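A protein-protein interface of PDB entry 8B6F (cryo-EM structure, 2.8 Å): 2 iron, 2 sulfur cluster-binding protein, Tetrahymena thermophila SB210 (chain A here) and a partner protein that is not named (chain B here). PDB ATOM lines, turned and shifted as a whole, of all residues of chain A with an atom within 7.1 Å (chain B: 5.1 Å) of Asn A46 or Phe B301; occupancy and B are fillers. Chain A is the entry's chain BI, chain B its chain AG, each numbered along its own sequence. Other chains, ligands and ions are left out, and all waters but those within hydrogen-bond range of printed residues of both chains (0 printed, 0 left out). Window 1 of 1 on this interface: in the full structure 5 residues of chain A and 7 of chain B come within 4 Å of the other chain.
N of Leu B294 sits close to NE2 of Gln B305 (3.3 Å).
The guanidinium group (NH1) of Arg A56 is in hydrogen-bond range of the side-chain amide oxygen (OD1) of Asn A46 (2.9 Å).
The backbone NH (N) of Asn A46 is in hydrogen-bond range of the backbone carbonyl oxygen (O) of Met A156 (2.9 Å).
N of Ile A158 is in hydrogen-bond range of O of Asn A46, 2.9 Å away.
The backbone carbonyl oxygen of Ile A47 sits at hydrogen-bond distance from the backbone NH of Glu A55 (2.9 Å).
OE1 of Glu A155 lies within salt-bridge range of NH1 of Arg A56 (3.0 Å).
Among the printed residues, pairs that only touch across the chains: Asn A46 with Pro B298, Ile A157 with Ser B300, Ile A157 with Phe B301, Phe A54 with Phe B301, Phe A54 with Leu B294, Asn A46 with Phe B301, Arg A56 with Phe B297, Ile A157 with Pro B298, Phe A54 with Tyr B304 and Glu A55 with Phe B297.
Asn A46 touches just these residues of chain B: Pro B298 (3.0 Å) and Phe B301 (3.6 Å).
Of the printed residues of chain A, Pro B298 touches Asn A46 (3.0 Å) and Ile A157 (3.8 Å).
Of chain A, only Asn A46, Phe A54 and Ile A157 come within 4 Å of Phe B301.
Printed residues of chain A within 4 Å of Tyr B304: Phe A54 (3.8 Å).
The nearest residue of chain B that does not touch Asn A46 is Phe B297 (4.5 Å).
The nearest residue of chain A that does not touch Phe B301 is Ile A47 (4.1 Å).
The nearest printed residue of chain A that does not touch Tyr B304 is Gln A48 (6.1 Å).
Of the 19 printed residues of chain A, 5 touch a printed residue of chain B.
Among the printed residues, 10 pairs touch across the chains.
Among the printed residues, no Asp or Glu carboxylate lies within 4 Å of a Lys or Arg side-chain nitrogen of the other chain.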
ATOM      1  N   TRP A  44       8.321   0.961 -11.691  1.00  0.00           N
ATOM      2  CA  TRP A  44       8.025   1.633 -12.948  1.00  0.00           C
ATOM      3  C   TRP A  44       7.173   0.744 -13.842  1.00  0.00           C
ATOM      4  O   TRP A  44       7.499  -0.427 -14.063  1.00  0.00           O
ATOM      5  CB  TRP A  44       9.317   2.026 -13.662  1.00  0.00           C
ATOM      6  CG  TRP A  44      10.044   3.139 -12.985  1.00  0.00           C
ATOM      7  CD1 TRP A  44      11.212   3.052 -12.290  1.00  0.00           C
ATOM      8  CD2 TRP A  44       9.646   4.512 -12.932  1.00  0.00           C
ATOM      9  NE1 TRP A  44      11.569   4.287 -11.811  1.00  0.00           N
ATOM     10  CE2 TRP A  44      10.622   5.201 -12.190  1.00  0.00           C
ATOM     11  CE3 TRP A  44       8.557   5.226 -13.440  1.00  0.00           C
ATOM     12  CZ2 TRP A  44      10.547   6.567 -11.950  1.00  0.00           C
ATOM     13  CZ3 TRP A  44       8.481   6.580 -13.200  1.00  0.00           C
ATOM     14  CH2 TRP A  44       9.470   7.239 -12.460  1.00  0.00           C
ATOM     15  N   ILE A  45       6.089   1.313 -14.362  1.00  0.00           N
ATOM     16  CA  ILE A  45       5.174   0.630 -15.267  1.00  0.00           C
ATOM     17  C   ILE A  45       5.189   1.370 -16.595  1.00  0.00           C
ATOM     18  O   ILE A  45       4.946   2.580 -16.639  1.00  0.00           O
ATOM     19  CB  ILE A  45       3.747   0.566 -14.692  1.00  0.00           C
ATOM     20  CG1 ILE A  45       3.741  -0.136 -13.330  1.00  0.00           C
ATOM     21  CG2 ILE A  45       2.807  -0.135 -15.663  1.00  0.00           C
ATOM     22  CD1 ILE A  45       4.214  -1.577 -13.362  1.00  0.00           C
ATOM     23  N   ASN A  46       5.467   0.642 -17.671  1.00  0.00           N
ATOM     24  CA  ASN A  46       5.491   1.201 -19.015  1.00  0.00           C
ATOM     25  C   ASN A  46       4.213   0.802 -19.738  1.00  0.00           C
ATOM     26  O   ASN A  46       3.808  -0.363 -19.695  1.00  0.00           O
ATOM     27  CB  ASN A  46       6.719   0.709 -19.782  1.00  0.00           C
ATOM     28  CG  ASN A  46       8.012   1.012 -19.056  1.00  0.00           C
ATOM     29  OD1 ASN A  46       8.213   2.118 -18.562  1.00  0.00           O
ATOM     30  ND2 ASN A  46       8.891   0.026 -18.979  1.00  0.00           N
ATOM     31  N   ILE A  47       3.585   1.770 -20.399  1.00  0.00           N
ATOM     32  CA  ILE A  47       2.253   1.610 -20.963  1.00  0.00           C
ATOM     33  C   ILE A  47       2.260   2.081 -22.408  1.00  0.00           C
ATOM     34  O   ILE A  47       2.931   3.060 -22.751  1.00  0.00           O
ATOM     35  CB  ILE A  47       1.203   2.396 -20.151  1.00  0.00           C
ATOM     36  CG1 ILE A  47       1.234   1.963 -18.683  1.00  0.00           C
ATOM     37  CG2 ILE A  47      -0.182   2.188 -20.739  1.00  0.00           C
ATOM     38  CD1 ILE A  47       0.406   2.835 -17.765  1.00  0.00           C
ATOM     39  N   GLN A  48       1.515   1.377 -23.257  1.00  0.00           N
ATOM     40  CA  GLN A  48       1.188   1.841 -24.600  1.00  0.00           C
ATOM     41  C   GLN A  48      -0.247   2.351 -24.566  1.00  0.00           C
ATOM     42  O   GLN A  48      -1.188   1.572 -24.385  1.00  0.00           O
ATOM     43  CB  GLN A  48       1.355   0.736 -25.638  1.00  0.00           C
ATOM     44  CG  GLN A  48       1.262   1.256 -27.064  1.00  0.00           C
ATOM     45  CD  GLN A  48       1.317   0.155 -28.094  1.00  0.00           C
ATOM     46  OE1 GLN A  48       1.074  -1.011 -27.788  1.00  0.00           O
ATOM     47  NE2 GLN A  48       1.636   0.519 -29.329  1.00  0.00           N
ATOM     48  N   GLN A  53       0.862   5.943 -28.240  1.00  0.00           N
ATOM     49  CA  GLN A  53       2.044   6.558 -27.660  1.00  0.00           C
ATOM     50  C   GLN A  53       2.492   5.777 -26.428  1.00  0.00           C
ATOM     51  O   GLN A  53       1.832   4.839 -25.980  1.00  0.00           O
ATOM     52  CB  GLN A  53       1.762   8.017 -27.313  1.00  0.00           C
ATOM     53  CG  GLN A  53       1.396   8.850 -28.525  1.00  0.00           C
ATOM     54  CD  GLN A  53       0.992  10.258 -28.161  1.00  0.00           C
ATOM     55  OE1 GLN A  53       1.395  10.784 -27.126  1.00  0.00           O
ATOM     56  NE2 GLN A  53       0.183  10.876 -29.011  1.00  0.00           N
ATOM     57  N   PHE A  54       3.628   6.184 -25.870  1.00  0.00           N
ATOM     58  CA  PHE A  54       4.246   5.488 -24.751  1.00  0.00           C
ATOM     59  C   PHE A  54       4.208   6.354 -23.502  1.00  0.00           C
ATOM     60  O   PHE A  54       4.435   7.566 -23.565  1.00  0.00           O
ATOM     61  CB  PHE A  54       5.694   5.113 -25.075  1.00  0.00           C
ATOM     62  CG  PHE A  54       5.835   4.249 -26.291  1.00  0.00           C
ATOM     63  CD1 PHE A  54       5.239   3.004 -26.342  1.00  0.00           C
ATOM     64  CD2 PHE A  54       6.572   4.678 -27.379  1.00  0.00           C
ATOM     65  CE1 PHE A  54       5.366   2.206 -27.459  1.00  0.00           C
ATOM     66  CE2 PHE A  54       6.704   3.884 -28.499  1.00  0.00           C
ATOM     67  CZ  PHE A  54       6.100   2.645 -28.538  1.00  0.00           C
ATOM     68  N   GLU A  55       3.922   5.723 -22.366  1.00  0.00           N
ATOM     69  CA  GLU A  55       3.863   6.401 -21.084  1.00  0.00           C
ATOM     70  C   GLU A  55       4.630   5.595 -20.048  1.00  0.00           C
ATOM     71  O   GLU A  55       4.765   4.375 -20.164  1.00  0.00           O
ATOM     72  CB  GLU A  55       2.416   6.593 -20.617  1.00  0.00           C
ATOM     73  CG  GLU A  55       1.509   7.209 -21.668  1.00  0.00           C
ATOM     74  CD  GLU A  55       0.121   7.500 -21.139  1.00  0.00           C
ATOM     75  OE1 GLU A  55      -0.042   7.567 -19.903  1.00  0.00           O
ATOM     76  OE2 GLU A  55      -0.808   7.660 -21.957  1.00  0.00           O
ATOM     77  N   ARG A  56       5.124   6.290 -19.028  1.00  0.00           N
ATOM     78  CA  ARG A  56       5.880   5.666 -17.951  1.00  0.00           C
ATOM     79  C   ARG A  56       5.393   6.249 -16.636  1.00  0.00           C
ATOM     80  O   ARG A  56       5.455   7.465 -16.437  1.00  0.00           O
ATOM     81  CB  ARG A  56       7.382   5.906 -18.130  1.00  0.00           C
ATOM     82  CG  ARG A  56       8.268   5.249 -17.086  1.00  0.00           C
ATOM     83  CD  ARG A  56       9.728   5.546 -17.382  1.00  0.00           C
ATOM     84  NE  ARG A  56      10.632   4.999 -16.378  1.00  0.00           N
ATOM     85  CZ  ARG A  56      11.095   3.757 -16.379  1.00  0.00           C
ATOM     86  NH1 ARG A  56      10.727   2.884 -17.301  1.00  0.00           N
ATOM     87  NH2 ARG A  56      11.949   3.382 -15.433  1.00  0.00           N
ATOM     88  N   ILE A  57       4.905   5.388 -15.745  1.00  0.00           N
ATOM     89  CA  ILE A  57       4.317   5.815 -14.485  1.00  0.00           C
ATOM     90  C   ILE A  57       4.973   5.040 -13.352  1.00  0.00           C
ATOM     91  O   ILE A  57       5.677   4.053 -13.567  1.00  0.00           O
ATOM     92  CB  ILE A  57       2.789   5.628 -14.452  1.00  0.00           C
ATOM     93  CG1 ILE A  57       2.438   4.145 -14.583  1.00  0.00           C
ATOM     94  CG2 ILE A  57       2.144   6.444 -15.564  1.00  0.00           C
ATOM     95  CD1 ILE A  57       0.976   3.859 -14.444  1.00  0.00           C
ATOM     96  N   VAL A 110      -3.653  -5.285 -21.296  1.00  0.00           N
ATOM     97  CA  VAL A 110      -2.900  -6.369 -21.917  1.00  0.00           C
ATOM     98  C   VAL A 110      -1.479  -6.323 -21.372  1.00  0.00           C
ATOM     99  O   VAL A 110      -0.784  -5.312 -21.519  1.00  0.00           O
ATOM    100  CB  VAL A 110      -2.912  -6.251 -23.448  1.00  0.00           C
ATOM    101  CG1 VAL A 110      -2.199  -7.433 -24.077  1.00  0.00           C
ATOM    102  CG2 VAL A 110      -4.336  -6.150 -23.963  1.00  0.00           C
ATOM    103  N   TRP A 115       5.766 -11.069 -17.856  1.00  0.00           N
ATOM    104  CA  TRP A 115       5.087 -10.826 -16.592  1.00  0.00           C
ATOM    105  C   TRP A 115       3.727 -11.503 -16.523  1.00  0.00           C
ATOM    106  O   TRP A 115       3.266 -11.835 -15.427  1.00  0.00           O
ATOM    107  CB  TRP A 115       4.927  -9.323 -16.360  1.00  0.00           C
ATOM    108  CG  TRP A 115       6.236  -8.606 -16.273  1.00  0.00           C
ATOM    109  CD1 TRP A 115       6.976  -8.388 -15.149  1.00  0.00           C
ATOM    110  CD2 TRP A 115       6.967  -8.021 -17.356  1.00  0.00           C
ATOM    111  NE1 TRP A 115       8.122  -7.702 -15.465  1.00  0.00           N
ATOM    112  CE2 TRP A 115       8.141  -7.464 -16.814  1.00  0.00           C
ATOM    113  CE3 TRP A 115       6.742  -7.914 -18.732  1.00  0.00           C
ATOM    114  CZ2 TRP A 115       9.086  -6.809 -17.598  1.00  0.00           C
ATOM    115  CZ3 TRP A 115       7.682  -7.263 -19.510  1.00  0.00           C
ATOM    116  CH2 TRP A 115       8.840  -6.718 -18.941  1.00  0.00           C
ATOM    117  N   MET A 153       7.351  -6.814 -10.746  1.00  0.00           N
ATOM    118  CA  MET A 153       6.690  -6.150 -11.861  1.00  0.00           C
ATOM    119  C   MET A 153       7.445  -4.923 -12.357  1.00  0.00           C
ATOM    120  O   MET A 153       6.937  -4.219 -13.234  1.00  0.00           O
ATOM    121  CB  MET A 153       5.271  -5.740 -11.462  1.00  0.00           C
ATOM    122  CG  MET A 153       4.353  -6.905 -11.157  1.00  0.00           C
ATOM    123  SD  MET A 153       2.683  -6.371 -10.757  1.00  0.00           S
ATOM    124  CE  MET A 153       1.898  -7.946 -10.441  1.00  0.00           C
ATOM    125  N   ASN A 154       8.632  -4.648 -11.822  1.00  0.00           N
ATOM    126  CA  ASN A 154       9.378  -3.467 -12.231  1.00  0.00           C
ATOM    127  C   ASN A 154       9.642  -3.501 -13.731  1.00  0.00           C
ATOM    128  O   ASN A 154      10.048  -4.529 -14.278  1.00  0.00           O
ATOM    129  CB  ASN A 154      10.695  -3.389 -11.461  1.00  0.00           C
ATOM    130  CG  ASN A 154      11.402  -2.067 -11.651  1.00  0.00           C
ATOM    131  OD1 ASN A 154      10.766  -1.025 -11.784  1.00  0.00           O
ATOM    132  ND2 ASN A 154      12.729  -2.104 -11.667  1.00  0.00           N
ATOM    133  N   GLU A 155       9.410  -2.369 -14.393  1.00  0.00           N
ATOM    134  CA  GLU A 155       9.591  -2.219 -15.832  1.00  0.00           C
ATOM    135  C   GLU A 155       8.598  -3.046 -16.638  1.00  0.00           C
ATOM    136  O   GLU A 155       8.844  -3.335 -17.812  1.00  0.00           O
ATOM    137  CB  GLU A 155      11.020  -2.586 -16.249  1.00  0.00           C
ATOM    138  CG  GLU A 155      12.101  -1.898 -15.430  1.00  0.00           C
ATOM    139  CD  GLU A 155      12.082  -0.392 -15.584  1.00  0.00           C
ATOM    140  OE1 GLU A 155      11.441   0.102 -16.534  1.00  0.00           O
ATOM    141  OE2 GLU A 155      12.705   0.299 -14.753  1.00  0.00           O
ATOM    142  N   MET A 156       7.478  -3.435 -16.038  1.00  0.00           N
ATOM    143  CA  MET A 156       6.485  -4.227 -16.749  1.00  0.00           C
ATOM    144  C   MET A 156       5.834  -3.409 -17.859  1.00  0.00           C
ATOM    145  O   MET A 156       5.461  -2.251 -17.662  1.00  0.00           O
ATOM    146  CB  MET A 156       5.418  -4.733 -15.780  1.00  0.00           C
ATOM    147  CG  MET A 156       4.312  -5.537 -16.449  1.00  0.00           C
ATOM    148  SD  MET A 156       3.182  -6.304 -15.271  1.00  0.00           S
ATOM    149  CE  MET A 156       2.478  -4.864 -14.473  1.00  0.00           C
ATOM    150  N   ILE A 157       5.697  -4.026 -19.029  1.00  0.00           N
ATOM    151  CA  ILE A 157       5.122  -3.383 -20.205  1.00  0.00           C
ATOM    152  C   ILE A 157       3.692  -3.873 -20.373  1.00  0.00           C
ATOM    153  O   ILE A 157       3.439  -5.083 -20.371  1.00  0.00           O
ATOM    154  CB  ILE A 157       5.954  -3.682 -21.463  1.00  0.00           C
ATOM    155  CG1 ILE A 157       7.371  -3.121 -21.308  1.00  0.00           C
ATOM    156  CG2 ILE A 157       5.274  -3.112 -22.698  1.00  0.00           C
ATOM    157  CD1 ILE A 157       8.323  -3.535 -22.413  1.00  0.00           C
ATOM    158  N   ILE A 158       2.755  -2.936 -20.520  1.00  0.00           N
ATOM    159  CA  ILE A 158       1.351  -3.252 -20.753  1.00  0.00           C
ATOM    160  C   ILE A 158       0.830  -2.342 -21.858  1.00  0.00           C
ATOM    161  O   ILE A 158       1.451  -1.341 -22.217  1.00  0.00           O
ATOM    162  CB  ILE A 158       0.490  -3.101 -19.480  1.00  0.00           C
ATOM    163  CG1 ILE A 158       0.423  -1.632 -19.049  1.00  0.00           C
ATOM    164  CG2 ILE A 158       1.054  -3.969 -18.364  1.00  0.00           C
ATOM    165  CD1 ILE A 158      -0.320  -1.389 -17.745  1.00  0.00           C
ATOM    166  N   SER A 159      -0.327  -2.708 -22.401  1.00  0.00           N
ATOM    167  CA  SER A 159      -1.039  -1.893 -23.373  1.00  0.00           C
ATOM    168  C   SER A 159      -2.451  -1.663 -22.862  1.00  0.00           C
ATOM    169  O   SER A 159      -3.045  -2.555 -22.252  1.00  0.00           O
ATOM    170  CB  SER A 159      -1.084  -2.560 -24.753  1.00  0.00           C
ATOM    171  OG  SER A 159       0.220  -2.812 -25.246  1.00  0.00           O
ATOM    172  N   LEU B 294      12.192   8.635 -25.679  1.00  0.00           N
ATOM    173  CA  LEU B 294      12.131   7.302 -25.098  1.00  0.00           C
ATOM    174  C   LEU B 294      13.374   6.953 -24.290  1.00  0.00           C
ATOM    175  O   LEU B 294      13.686   5.769 -24.128  1.00  0.00           O
ATOM    176  CB  LEU B 294      11.893   6.263 -26.193  1.00  0.00           C
ATOM    177  CG  LEU B 294      10.596   6.452 -26.989  1.00  0.00           C
ATOM    178  CD1 LEU B 294      10.406   5.314 -27.964  1.00  0.00           C
ATOM    179  CD2 LEU B 294       9.379   6.571 -26.081  1.00  0.00           C
ATOM    180  N   PHE B 297      13.136   4.391 -21.186  1.00  0.00           N
ATOM    181  CA  PHE B 297      12.137   3.399 -21.554  1.00  0.00           C
ATOM    182  C   PHE B 297      12.812   2.103 -21.971  1.00  0.00           C
ATOM    183  O   PHE B 297      14.019   2.060 -22.219  1.00  0.00           O
ATOM    184  CB  PHE B 297      11.260   3.945 -22.677  1.00  0.00           C
ATOM    185  CG  PHE B 297      10.298   5.006 -22.232  1.00  0.00           C
ATOM    186  CD1 PHE B 297      10.742   6.281 -21.923  1.00  0.00           C
ATOM    187  CD2 PHE B 297       8.946   4.733 -22.134  1.00  0.00           C
ATOM    188  CE1 PHE B 297       9.855   7.260 -21.520  1.00  0.00           C
ATOM    189  CE2 PHE B 297       8.056   5.705 -21.731  1.00  0.00           C
ATOM    190  CZ  PHE B 297       8.511   6.972 -21.424  1.00  0.00           C
ATOM    191  N   PRO B 298      12.057   1.009 -22.058  1.00  0.00           N
ATOM    192  CA  PRO B 298      12.652  -0.265 -22.474  1.00  0.00           C
ATOM    193  C   PRO B 298      13.188  -0.202 -23.897  1.00  0.00           C
ATOM    194  O   PRO B 298      12.805   0.649 -24.701  1.00  0.00           O
ATOM    195  CB  PRO B 298      11.488  -1.258 -22.366  1.00  0.00           C
ATOM    196  CG  PRO B 298      10.523  -0.622 -21.442  1.00  0.00           C
ATOM    197  CD  PRO B 298      10.646   0.851 -21.665  1.00  0.00           C
ATOM    198  N   ASP B 299      14.095  -1.132 -24.201  1.00  0.00           N
ATOM    199  CA  ASP B 299      14.654  -1.203 -25.547  1.00  0.00           C
ATOM    200  C   ASP B 299      13.574  -1.471 -26.585  1.00  0.00           C
ATOM    201  O   ASP B 299      13.669  -0.988 -27.719  1.00  0.00           O
ATOM    202  CB  ASP B 299      15.726  -2.290 -25.618  1.00  0.00           C
ATOM    203  CG  ASP B 299      16.796  -2.118 -24.563  1.00  0.00           C
ATOM    204  OD1 ASP B 299      16.996  -0.977 -24.101  1.00  0.00           O
ATOM    205  OD2 ASP B 299      17.440  -3.124 -24.197  1.00  0.00           O
ATOM    206  N   SER B 300      12.549  -2.244 -26.224  1.00  0.00           N
ATOM    207  CA  SER B 300      11.460  -2.505 -27.159  1.00  0.00           C
ATOM    208  C   SER B 300      10.767  -1.211 -27.560  1.00  0.00           C
ATOM    209  O   SER B 300      10.450  -1.006 -28.737  1.00  0.00           O
ATOM    210  CB  SER B 300      10.465  -3.484 -26.539  1.00  0.00           C
ATOM    211  OG  SER B 300       9.993  -3.007 -25.292  1.00  0.00           O
ATOM    212  N   PHE B 301      10.515  -0.328 -26.593  1.00  0.00           N
ATOM    213  CA  PHE B 301       9.950   0.978 -26.915  1.00  0.00           C
ATOM    214  C   PHE B 301      10.945   1.833 -27.689  1.00  0.00           C
ATOM    215  O   PHE B 301      10.575   2.484 -28.671  1.00  0.00           O
ATOM    216  CB  PHE B 301       9.508   1.695 -25.639  1.00  0.00           C
ATOM    217  CG  PHE B 301       8.265   1.120 -25.013  1.00  0.00           C
ATOM    218  CD1 PHE B 301       7.689  -0.044 -25.494  1.00  0.00           C
ATOM    219  CD2 PHE B 301       7.661   1.765 -23.949  1.00  0.00           C
ATOM    220  CE1 PHE B 301       6.546  -0.554 -24.919  1.00  0.00           C
ATOM    221  CE2 PHE B 301       6.519   1.257 -23.370  1.00  0.00           C
ATOM    222  CZ  PHE B 301       5.961   0.099 -23.856  1.00  0.00           C
ATOM    223  N   LYS B 302      12.213   1.833 -27.272  1.00  0.00           N
ATOM    224  CA  LYS B 302      13.218   2.634 -27.964  1.00  0.00           C
ATOM    225  C   LYS B 302      13.333   2.243 -29.431  1.00  0.00           C
ATOM    226  O   LYS B 302      13.753   3.058 -30.259  1.00  0.00           O
ATOM    227  CB  LYS B 302      14.574   2.489 -27.274  1.00  0.00           C
ATOM    228  CG  LYS B 302      14.665   3.175 -25.923  1.00  0.00           C
ATOM    229  CD  LYS B 302      16.053   3.015 -25.325  1.00  0.00           C
ATOM    230  CE  LYS B 302      16.200   3.819 -24.045  1.00  0.00           C
ATOM    231  NZ  LYS B 302      17.562   3.685 -23.460  1.00  0.00           N
ATOM    232  N   ALA B 303      12.976   1.004 -29.770  1.00  0.00           N
ATOM    233  CA  ALA B 303      13.019   0.581 -31.165  1.00  0.00           C
ATOM    234  C   ALA B 303      12.154   1.471 -32.048  1.00  0.00           C
ATOM    235  O   ALA B 303      12.413   1.586 -33.251  1.00  0.00           O
ATOM    236  CB  ALA B 303      12.574  -0.875 -31.286  1.00  0.00           C
ATOM    237  N   TYR B 304      11.130   2.101 -31.480  1.00  0.00           N
ATOM    238  CA  TYR B 304      10.242   2.983 -32.227  1.00  0.00           C
ATOM    239  C   TYR B 304      10.728   4.426 -32.267  1.00  0.00           C
ATOM    240  O   TYR B 304      10.091   5.259 -32.917  1.00  0.00           O
ATOM    241  CB  TYR B 304       8.835   2.934 -31.626  1.00  0.00           C
ATOM    242  CG  TYR B 304       8.131   1.619 -31.859  1.00  0.00           C
ATOM    243  CD1 TYR B 304       7.363   1.414 -32.996  1.00  0.00           C
ATOM    244  CD2 TYR B 304       8.233   0.583 -30.942  1.00  0.00           C
ATOM    245  CE1 TYR B 304       6.719   0.215 -33.216  1.00  0.00           C
ATOM    246  CE2 TYR B 304       7.593  -0.620 -31.152  1.00  0.00           C
ATOM    247  CZ  TYR B 304       6.837  -0.797 -32.290  1.00  0.00           C
ATOM    248  OH  TYR B 304       6.193  -1.993 -32.506  1.00  0.00           O
ATOM    249  N   GLN B 305      11.826   4.740 -31.589  1.00  0.00           N
ATOM    250  CA  GLN B 305      12.391   6.076 -31.646  1.00  0.00           C
ATOM    251  C   GLN B 305      13.018   6.326 -33.017  1.00  0.00           C
ATOM    252  O   GLN B 305      13.407   5.398 -33.731  1.00  0.00           O
ATOM    253  CB  GLN B 305      13.437   6.251 -30.543  1.00  0.00           C
ATOM    254  CG  GLN B 305      14.055   7.641 -30.451  1.00  0.00           C
ATOM    255  CD  GLN B 305      13.056   8.705 -30.048  1.00  0.00           C
ATOM    256  OE1 GLN B 305      12.917   9.727 -30.717  1.00  0.00           O
ATOM    257  NE2 GLN B 305      12.369   8.480 -28.938  1.00  0.00           N
